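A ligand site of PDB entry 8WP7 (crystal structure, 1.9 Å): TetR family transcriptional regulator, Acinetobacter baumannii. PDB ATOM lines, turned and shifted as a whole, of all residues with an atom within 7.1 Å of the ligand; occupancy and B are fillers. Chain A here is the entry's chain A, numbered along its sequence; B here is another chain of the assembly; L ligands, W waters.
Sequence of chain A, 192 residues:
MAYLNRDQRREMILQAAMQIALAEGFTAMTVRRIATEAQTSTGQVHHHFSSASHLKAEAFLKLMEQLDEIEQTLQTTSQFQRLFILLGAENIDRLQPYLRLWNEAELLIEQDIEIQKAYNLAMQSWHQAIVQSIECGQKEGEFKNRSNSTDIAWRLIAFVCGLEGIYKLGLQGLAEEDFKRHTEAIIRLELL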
ATOM      1  N   MET A  64      18.282  -4.569 -13.651  1.00  0.00           N
ATOM      2  CA  MET A  64      19.111  -4.188 -14.788  1.00  0.00           C
ATOM      3  C   MET A  64      20.365  -5.043 -14.872  1.00  0.00           C
ATOM      4  O   MET A  64      20.796  -5.425 -15.962  1.00  0.00           O
ATOM      5  CB  MET A  64      19.453  -2.693 -14.708  1.00  0.00           C
ATOM      6  CG  MET A  64      18.267  -1.770 -15.014  1.00  0.00           C
ATOM      7  SD  MET A  64      17.309  -2.185 -16.505  1.00  0.00           S
ATOM      8  CE  MET A  64      15.865  -2.999 -15.824  1.00  0.00           C
ATOM      9  N   LEU A  67      19.214  -8.111 -16.362  1.00  0.00           N
ATOM     10  CA  LEU A  67      19.136  -7.984 -17.819  1.00  0.00           C
ATOM     11  C   LEU A  67      20.515  -8.128 -18.449  1.00  0.00           C
ATOM     12  O   LEU A  67      20.658  -8.778 -19.492  1.00  0.00           O
ATOM     13  CB  LEU A  67      18.502  -6.638 -18.185  1.00  0.00           C
ATOM     14  CG  LEU A  67      18.780  -6.030 -19.571  1.00  0.00           C
ATOM     15  CD1 LEU A  67      18.360  -6.958 -20.693  1.00  0.00           C
ATOM     16  CD2 LEU A  67      18.125  -4.665 -19.725  1.00  0.00           C
ATOM     17  N   ASP A  68      21.532  -7.537 -17.832  1.00  0.00           N
ATOM     18  CA  ASP A  68      22.909  -7.723 -18.284  1.00  0.00           C
ATOM     19  C   ASP A  68      23.273  -9.199 -18.325  1.00  0.00           C
ATOM     20  O   ASP A  68      23.801  -9.698 -19.328  1.00  0.00           O
ATOM     21  CB  ASP A  68      23.868  -6.970 -17.366  1.00  0.00           C
ATOM     22  CG  ASP A  68      23.832  -5.464 -17.589  1.00  0.00           C
ATOM     23  OD1 ASP A  68      22.996  -5.006 -18.391  1.00  0.00           O
ATOM     24  OD2 ASP A  68      24.640  -4.749 -16.954  1.00  0.00           O
ATOM     25  N   GLU A  71      21.469 -11.013 -21.147  1.00  0.00           N
ATOM     26  CA  GLU A  71      22.040 -10.671 -22.441  1.00  0.00           C
ATOM     27  C   GLU A  71      23.358 -11.409 -22.679  1.00  0.00           C
ATOM     28  O   GLU A  71      23.683 -11.720 -23.833  1.00  0.00           O
ATOM     29  CB  GLU A  71      22.271  -9.162 -22.530  1.00  0.00           C
ATOM     30  CG  GLU A  71      21.022  -8.360 -22.889  1.00  0.00           C
ATOM     31  CD  GLU A  71      21.297  -6.873 -22.938  1.00  0.00           C
ATOM     32  OE1 GLU A  71      20.482  -6.129 -23.537  1.00  0.00           O
ATOM     33  OE2 GLU A  71      22.333  -6.442 -22.395  1.00  0.00           O
ATOM     34  N   ILE A  85      22.899  -6.490 -29.553  1.00  0.00           N
ATOM     35  CA  ILE A  85      22.158  -6.889 -28.361  1.00  0.00           C
ATOM     36  C   ILE A  85      22.225  -5.783 -27.318  1.00  0.00           C
ATOM     37  O   ILE A  85      21.196  -5.359 -26.778  1.00  0.00           O
ATOM     38  CB  ILE A  85      22.713  -8.221 -27.812  1.00  0.00           C
ATOM     39  CG1 ILE A  85      22.316  -9.370 -28.740  1.00  0.00           C
ATOM     40  CG2 ILE A  85      22.182  -8.470 -26.405  1.00  0.00           C
ATOM     41  CD1 ILE A  85      23.049 -10.668 -28.466  1.00  0.00           C
ATOM     42  N   LEU A  86      23.437  -5.283 -27.034  1.00  0.00           N
ATOM     43  CA  LEU A  86      23.598  -4.223 -26.038  1.00  0.00           C
ATOM     44  C   LEU A  86      22.796  -2.978 -26.398  1.00  0.00           C
ATOM     45  O   LEU A  86      22.284  -2.294 -25.504  1.00  0.00           O
ATOM     46  CB  LEU A  86      25.075  -3.886 -25.880  1.00  0.00           C
ATOM     47  CG  LEU A  86      25.927  -4.786 -24.989  1.00  0.00           C
ATOM     48  CD1 LEU A  86      27.405  -4.453 -25.174  1.00  0.00           C
ATOM     49  CD2 LEU A  86      25.530  -4.637 -23.523  1.00  0.00           C
ATOM     50  N   LEU A  87      22.694  -2.653 -27.680  1.00  0.00           N
ATOM     51  CA  LEU A  87      21.979  -1.457 -28.109  1.00  0.00           C
ATOM     52  C   LEU A  87      20.482  -1.687 -28.329  1.00  0.00           C
ATOM     53  O   LEU A  87      19.793  -0.755 -28.770  1.00  0.00           O
ATOM     54  CB  LEU A  87      22.610  -0.899 -29.401  1.00  0.00           C
ATOM     55  CG  LEU A  87      24.044  -0.401 -29.256  1.00  0.00           C
ATOM     56  CD1 LEU A  87      24.643  -0.117 -30.618  1.00  0.00           C
ATOM     57  CD2 LEU A  87      24.063   0.868 -28.399  1.00  0.00           C
ATOM     58  N   GLY A  88      19.968  -2.873 -28.040  1.00  0.00           N
ATOM     59  CA  GLY A  88      18.536  -3.103 -28.116  1.00  0.00           C
ATOM     60  C   GLY A  88      17.995  -3.331 -29.501  1.00  0.00           C
ATOM     61  O   GLY A  88      16.770  -3.276 -29.684  1.00  0.00           O
ATOM     62  N   LEU A  95      13.157  -9.897 -22.807  1.00  0.00           N
ATOM     63  CA  LEU A  95      13.600  -8.652 -22.181  1.00  0.00           C
ATOM     64  C   LEU A  95      12.544  -7.559 -22.183  1.00  0.00           C
ATOM     65  O   LEU A  95      12.757  -6.516 -21.550  1.00  0.00           O
ATOM     66  CB  LEU A  95      14.861  -8.145 -22.872  1.00  0.00           C
ATOM     67  CG  LEU A  95      15.954  -9.185 -23.136  1.00  0.00           C
ATOM     68  CD1 LEU A  95      17.169  -8.559 -23.784  1.00  0.00           C
ATOM     69  CD2 LEU A  95      16.322  -9.865 -21.833  1.00  0.00           C
ATOM     70  N   TYR A  98      11.733  -5.966 -18.908  1.00  0.00           N
ATOM     71  CA  TYR A  98      12.858  -5.169 -18.417  1.00  0.00           C
ATOM     72  C   TYR A  98      12.937  -3.842 -19.160  1.00  0.00           C
ATOM     73  O   TYR A  98      13.237  -2.802 -18.568  1.00  0.00           O
ATOM     74  CB  TYR A  98      14.174  -5.932 -18.558  1.00  0.00           C
ATOM     75  CG  TYR A  98      14.280  -7.211 -17.755  1.00  0.00           C
ATOM     76  CD1 TYR A  98      13.599  -8.356 -18.158  1.00  0.00           C
ATOM     77  CD2 TYR A  98      15.061  -7.274 -16.611  1.00  0.00           C
ATOM     78  CE1 TYR A  98      13.705  -9.535 -17.436  1.00  0.00           C
ATOM     79  CE2 TYR A  98      15.169  -8.441 -15.876  1.00  0.00           C
ATOM     80  CZ  TYR A  98      14.490  -9.578 -16.295  1.00  0.00           C
ATOM     81  OH  TYR A  98      14.584 -10.745 -15.575  1.00  0.00           O
ATOM     82  N   LEU A  99      12.702  -3.868 -20.472  1.00  0.00           N
ATOM     83  CA  LEU A  99      12.742  -2.657 -21.276  1.00  0.00           C
ATOM     84  C   LEU A  99      11.550  -1.755 -20.962  1.00  0.00           C
ATOM     85  O   LEU A  99      11.686  -0.520 -21.007  1.00  0.00           O
ATOM     86  CB  LEU A  99      12.772  -3.017 -22.757  1.00  0.00           C
ATOM     87  CG  LEU A  99      14.023  -3.785 -23.192  1.00  0.00           C
ATOM     88  CD1 LEU A  99      13.944  -4.187 -24.669  1.00  0.00           C
ATOM     89  CD2 LEU A  99      15.290  -2.977 -22.915  1.00  0.00           C
ATOM     90  N   TRP A 102      12.658  -0.033 -17.793  1.00  0.00           N
ATOM     91  CA  TRP A 102      13.641   1.003 -18.083  1.00  0.00           C
ATOM     92  C   TRP A 102      12.949   2.268 -18.573  1.00  0.00           C
ATOM     93  O   TRP A 102      13.232   3.375 -18.099  1.00  0.00           O
ATOM     94  CB  TRP A 102      14.644   0.493 -19.119  1.00  0.00           C
ATOM     95  CG  TRP A 102      15.641   1.523 -19.558  1.00  0.00           C
ATOM     96  CD1 TRP A 102      15.415   2.623 -20.334  1.00  0.00           C
ATOM     97  CD2 TRP A 102      17.038   1.542 -19.233  1.00  0.00           C
ATOM     98  NE1 TRP A 102      16.579   3.336 -20.509  1.00  0.00           N
ATOM     99  CE2 TRP A 102      17.596   2.689 -19.836  1.00  0.00           C
ATOM    100  CE3 TRP A 102      17.872   0.706 -18.475  1.00  0.00           C
ATOM    101  CZ2 TRP A 102      18.943   3.011 -19.735  1.00  0.00           C
ATOM    102  CZ3 TRP A 102      19.212   1.030 -18.367  1.00  0.00           C
ATOM    103  CH2 TRP A 102      19.736   2.180 -18.993  1.00  0.00           C
ATOM    104  N   ASN A 103      12.023   2.131 -19.529  1.00  0.00           N
ATOM    105  CA  ASN A 103      11.306   3.294 -20.038  1.00  0.00           C
ATOM    106  C   ASN A 103      10.469   3.937 -18.949  1.00  0.00           C
ATOM    107  O   ASN A 103      10.347   5.167 -18.877  1.00  0.00           O
ATOM    108  CB  ASN A 103      10.430   2.894 -21.221  1.00  0.00           C
ATOM    109  CG  ASN A 103      11.236   2.631 -22.481  1.00  0.00           C
ATOM    110  OD1 ASN A 103      12.154   3.374 -22.809  1.00  0.00           O
ATOM    111  ND2 ASN A 103      10.880   1.570 -23.200  1.00  0.00           N
ATOM    112  N   GLU A 106      12.716   6.006 -16.770  1.00  0.00           N
ATOM    113  CA  GLU A 106      13.098   7.237 -17.441  1.00  0.00           C
ATOM    114  C   GLU A 106      12.128   8.373 -17.140  1.00  0.00           C
ATOM    115  O   GLU A 106      12.545   9.530 -17.024  1.00  0.00           O
ATOM    116  CB  GLU A 106      13.190   7.014 -18.951  1.00  0.00           C
ATOM    117  CG  GLU A 106      14.119   7.993 -19.655  1.00  0.00           C
ATOM    118  CD  GLU A 106      14.105   7.822 -21.162  1.00  0.00           C
ATOM    119  OE1 GLU A 106      13.636   6.760 -21.639  1.00  0.00           O
ATOM    120  OE2 GLU A 106      14.556   8.747 -21.859  1.00  0.00           O
ATOM    121  N   TYR A 119      18.837   5.618 -12.213  1.00  0.00           N
ATOM    122  CA  TYR A 119      18.791   5.645 -13.674  1.00  0.00           C
ATOM    123  C   TYR A 119      20.139   6.061 -14.255  1.00  0.00           C
ATOM    124  O   TYR A 119      20.590   5.495 -15.256  1.00  0.00           O
ATOM    125  CB  TYR A 119      17.698   6.594 -14.162  1.00  0.00           C
ATOM    126  CG  TYR A 119      17.461   6.550 -15.650  1.00  0.00           C
ATOM    127  CD1 TYR A 119      16.652   5.567 -16.219  1.00  0.00           C
ATOM    128  CD2 TYR A 119      18.061   7.463 -16.501  1.00  0.00           C
ATOM    129  CE1 TYR A 119      16.442   5.508 -17.583  1.00  0.00           C
ATOM    130  CE2 TYR A 119      17.854   7.411 -17.880  1.00  0.00           C
ATOM    131  CZ  TYR A 119      17.044   6.435 -18.407  1.00  0.00           C
ATOM    132  OH  TYR A 119      16.827   6.376 -19.778  1.00  0.00           O
ATOM    133  N   ALA A 122      22.614   3.196 -14.023  1.00  0.00           N
ATOM    134  CA  ALA A 122      22.389   2.212 -15.068  1.00  0.00           C
ATOM    135  C   ALA A 122      22.857   2.727 -16.428  1.00  0.00           C
ATOM    136  O   ALA A 122      23.325   1.938 -17.256  1.00  0.00           O
ATOM    137  CB  ALA A 122      20.914   1.830 -15.119  1.00  0.00           C
ATOM    138  N   MET A 123      22.721   4.032 -16.670  1.00  0.00           N
ATOM    139  CA  MET A 123      23.229   4.599 -17.916  1.00  0.00           C
ATOM    140  C   MET A 123      24.741   4.514 -17.973  1.00  0.00           C
ATOM    141  O   MET A 123      25.313   4.204 -19.029  1.00  0.00           O
ATOM    142  CB  MET A 123      22.764   6.062 -18.069  1.00  0.00           C
ATOM    143  CG  MET A 123      21.295   6.196 -18.421  1.00  0.00           C
ATOM    144  SD  MET A 123      20.914   5.880 -20.161  1.00  0.00           S
ATOM    145  CE  MET A 123      22.310   6.676 -20.948  1.00  0.00           C
ATOM    146  N   TRP A 126      25.622   0.911 -18.710  1.00  0.00           N
ATOM    147  CA  TRP A 126      25.385   0.643 -20.119  1.00  0.00           C
ATOM    148  C   TRP A 126      26.534   1.167 -20.965  1.00  0.00           C
ATOM    149  O   TRP A 126      27.042   0.463 -21.856  1.00  0.00           O
ATOM    150  CB  TRP A 126      24.062   1.297 -20.533  1.00  0.00           C
ATOM    151  CG  TRP A 126      23.559   0.959 -21.913  1.00  0.00           C
ATOM    152  CD1 TRP A 126      23.894  -0.116 -22.688  1.00  0.00           C
ATOM    153  CD2 TRP A 126      22.611   1.723 -22.675  1.00  0.00           C
ATOM    154  NE1 TRP A 126      23.215  -0.061 -23.886  1.00  0.00           N
ATOM    155  CE2 TRP A 126      22.422   1.053 -23.901  1.00  0.00           C
ATOM    156  CE3 TRP A 126      21.908   2.922 -22.445  1.00  0.00           C
ATOM    157  CZ2 TRP A 126      21.556   1.527 -24.893  1.00  0.00           C
ATOM    158  CZ3 TRP A 126      21.046   3.386 -23.428  1.00  0.00           C
ATOM    159  CH2 TRP A 126      20.882   2.694 -24.635  1.00  0.00           C
ATOM    160  N   ILE A 130      29.228  -1.034 -23.350  1.00  0.00           N
ATOM    161  CA  ILE A 130      29.482  -0.767 -24.773  1.00  0.00           C
ATOM    162  C   ILE A 130      30.956  -0.471 -24.995  1.00  0.00           C
ATOM    163  O   ILE A 130      31.550  -0.919 -25.991  1.00  0.00           O
ATOM    164  CB  ILE A 130      28.575   0.384 -25.255  1.00  0.00           C
ATOM    165  CG1 ILE A 130      27.118  -0.088 -25.269  1.00  0.00           C
ATOM    166  CG2 ILE A 130      28.994   0.851 -26.651  1.00  0.00           C
ATOM    167  CD1 ILE A 130      26.135   1.029 -25.489  1.00  0.00           C
ATOM    168  N   ILE A 157      25.019   5.319 -27.875  1.00  0.00           N
ATOM    169  CA  ILE A 157      23.899   5.464 -26.938  1.00  0.00           C
ATOM    170  C   ILE A 157      23.020   6.635 -27.337  1.00  0.00           C
ATOM    171  O   ILE A 157      21.785   6.523 -27.350  1.00  0.00           O
ATOM    172  CB  ILE A 157      24.431   5.619 -25.506  1.00  0.00           C
ATOM    173  CG1 ILE A 157      24.829   4.258 -24.934  1.00  0.00           C
ATOM    174  CG2 ILE A 157      23.376   6.281 -24.611  1.00  0.00           C
ATOM    175  CD1 ILE A 157      25.625   4.359 -23.652  1.00  0.00           C
ATOM    176  N   VAL A 160      20.718   5.582 -30.425  1.00  0.00           N
ATOM    177  CA  VAL A 160      19.572   4.697 -30.214  1.00  0.00           C
ATOM    178  C   VAL A 160      18.545   5.356 -29.304  1.00  0.00           C
ATOM    179  O   VAL A 160      17.331   5.190 -29.501  1.00  0.00           O
ATOM    180  CB  VAL A 160      20.019   3.318 -29.689  1.00  0.00           C
ATOM    181  CG1 VAL A 160      20.992   2.660 -30.657  1.00  0.00           C
ATOM    182  CG2 VAL A 160      20.667   3.422 -28.310  1.00  0.00           C
ATOM    183  N   CYS A 161      18.992   6.126 -28.305  1.00  0.00           N
ATOM    184  CA  CYS A 161      18.034   6.861 -27.486  1.00  0.00           C
ATOM    185  C   CYS A 161      17.299   7.915 -28.307  1.00  0.00           C
ATOM    186  O   CYS A 161      16.084   8.084 -28.158  1.00  0.00           O
ATOM    187  CB  CYS A 161      18.723   7.505 -26.289  1.00  0.00           C
ATOM    188  SG  CYS A 161      19.383   6.341 -25.086  1.00  0.00           S
ATOM    189  N   GLY A 162      18.022   8.629 -29.165  1.00  0.00           N
ATOM    190  CA  GLY A 162      17.379   9.632 -30.004  1.00  0.00           C
ATOM    191  C   GLY A 162      16.429   9.027 -31.011  1.00  0.00           C
ATOM    192  O   GLY A 162      15.381   9.596 -31.313  1.00  0.00           O
ATOM    193  N   GLU A 164      14.703   6.133 -30.706  1.00  0.00           N
ATOM    194  CA  GLU A 164      13.501   5.768 -29.958  1.00  0.00           C
ATOM    195  C   GLU A 164      12.660   6.991 -29.612  1.00  0.00           C
ATOM    196  O   GLU A 164      11.425   6.921 -29.624  1.00  0.00           O
ATOM    197  CB  GLU A 164      13.889   5.028 -28.687  1.00  0.00           C
ATOM    198  CG  GLU A 164      14.752   3.801 -28.903  1.00  0.00           C
ATOM    199  CD  GLU A 164      15.439   3.367 -27.620  1.00  0.00           C
ATOM    200  OE1 GLU A 164      16.486   2.685 -27.701  1.00  0.00           O
ATOM    201  OE2 GLU A 164      14.939   3.730 -26.536  1.00  0.00           O
ATOM    202  N   ILE B 166      20.700  13.030 -23.630  1.00  0.00           N
ATOM    203  CA  ILE B 166      21.670  12.476 -22.695  1.00  0.00           C
ATOM    204  C   ILE B 166      22.272  13.586 -21.835  1.00  0.00           C
ATOM    205  O   ILE B 166      22.522  13.384 -20.635  1.00  0.00           O
ATOM    206  CB  ILE B 166      22.759  11.713 -23.471  1.00  0.00           C
ATOM    207  CG1 ILE B 166      22.174  10.442 -24.102  1.00  0.00           C
ATOM    208  CG2 ILE B 166      23.860  11.288 -22.547  1.00  0.00           C
ATOM    209  CD1 ILE B 166      21.536   9.518 -23.107  1.00  0.00           C
HETATM  210  N1  LIG L   1      21.047  -3.305 -22.885  1.00  0.00           N
HETATM  211  C1  LIG L   1      20.424  -1.987 -22.974  1.00  0.00           C
HETATM  212  C2  LIG L   1      20.137  -1.439 -21.580  1.00  0.00           C
HETATM  213  C3  LIG L   1      18.762  -0.759 -21.576  1.00  0.00           C
HETATM  214  C4  LIG L   1      18.515  -0.055 -22.910  1.00  0.00           C
HETATM  215  N2  LIG L   1      17.587   1.048 -22.703  1.00  0.00           N
HETATM  216  C5  LIG L   1      16.810   1.276 -23.904  1.00  0.00           C
HETATM  217  C6  LIG L   1      16.078   2.605 -23.795  1.00  0.00           C
HETATM  218  C7  LIG L   1      17.082   3.749 -23.967  1.00  0.00           C
HETATM  219  N3  LIG L   1      16.482   4.990 -23.490  1.00  0.00           N
HETATM  220  O   HOH W   1      18.198   0.997 -26.677  1.00  0.00           O
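The indole nitrogen (NE1) of Trp 102 lies close to a nitrogen (N2) of the ligand (3.3 Å). N3 of the ligand is in salt-bridge range of OE2 of Glu 164 (3.6 Å). The side-chain carboxylate (OE1) of Glu 71 lies within salt-bridge range of a nitrogen (N1) of the ligand (3.0 Å). The side-chain carboxylate (OE1) of Glu 106 lies within salt-bridge range of a nitrogen (N3) of the ligand. A nitrogen (N1) of the ligand is in hydrogen-bond range of the backbone carbonyl oxygen (O) of Leu 86, at 3.1 Å. The side-chain sulfur of Cys 161 is in hydrogen-bond range of a nitrogen (N3) of the ligand.
The indole nitrogen (NE1) of Trp 102 is in hydrogen-bond range of the side-chain hydroxyl (OH) of Tyr 119. The backbone carbonyl oxygen (O) of Leu 86 lies within hydrogen-bond range of the indole nitrogen (NE1) of Trp 126, at 2.9 Å. The side-chain sulfur (SG) of Cys 161 is in hydrogen-bond range of the backbone carbonyl oxygen (O) of Ile 157.
Residues that only touch the ligand: Tyr 119 (3.98 Å) and Trp 126 (3.5 Å). Hydrophobic or aromatic side chains that line the ligand: Trp 102 and Trp 126. Within 4 Å of the ligand: Glu 71, Leu 86, Trp 102, Glu 106, Tyr 119, Trp 126, Cys 161 and Glu 164.
Water W1 lies within hydrogen-bond range of OE1 of Glu 164 (2.6 Å) and O of Leu 87 (3.2 Å).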
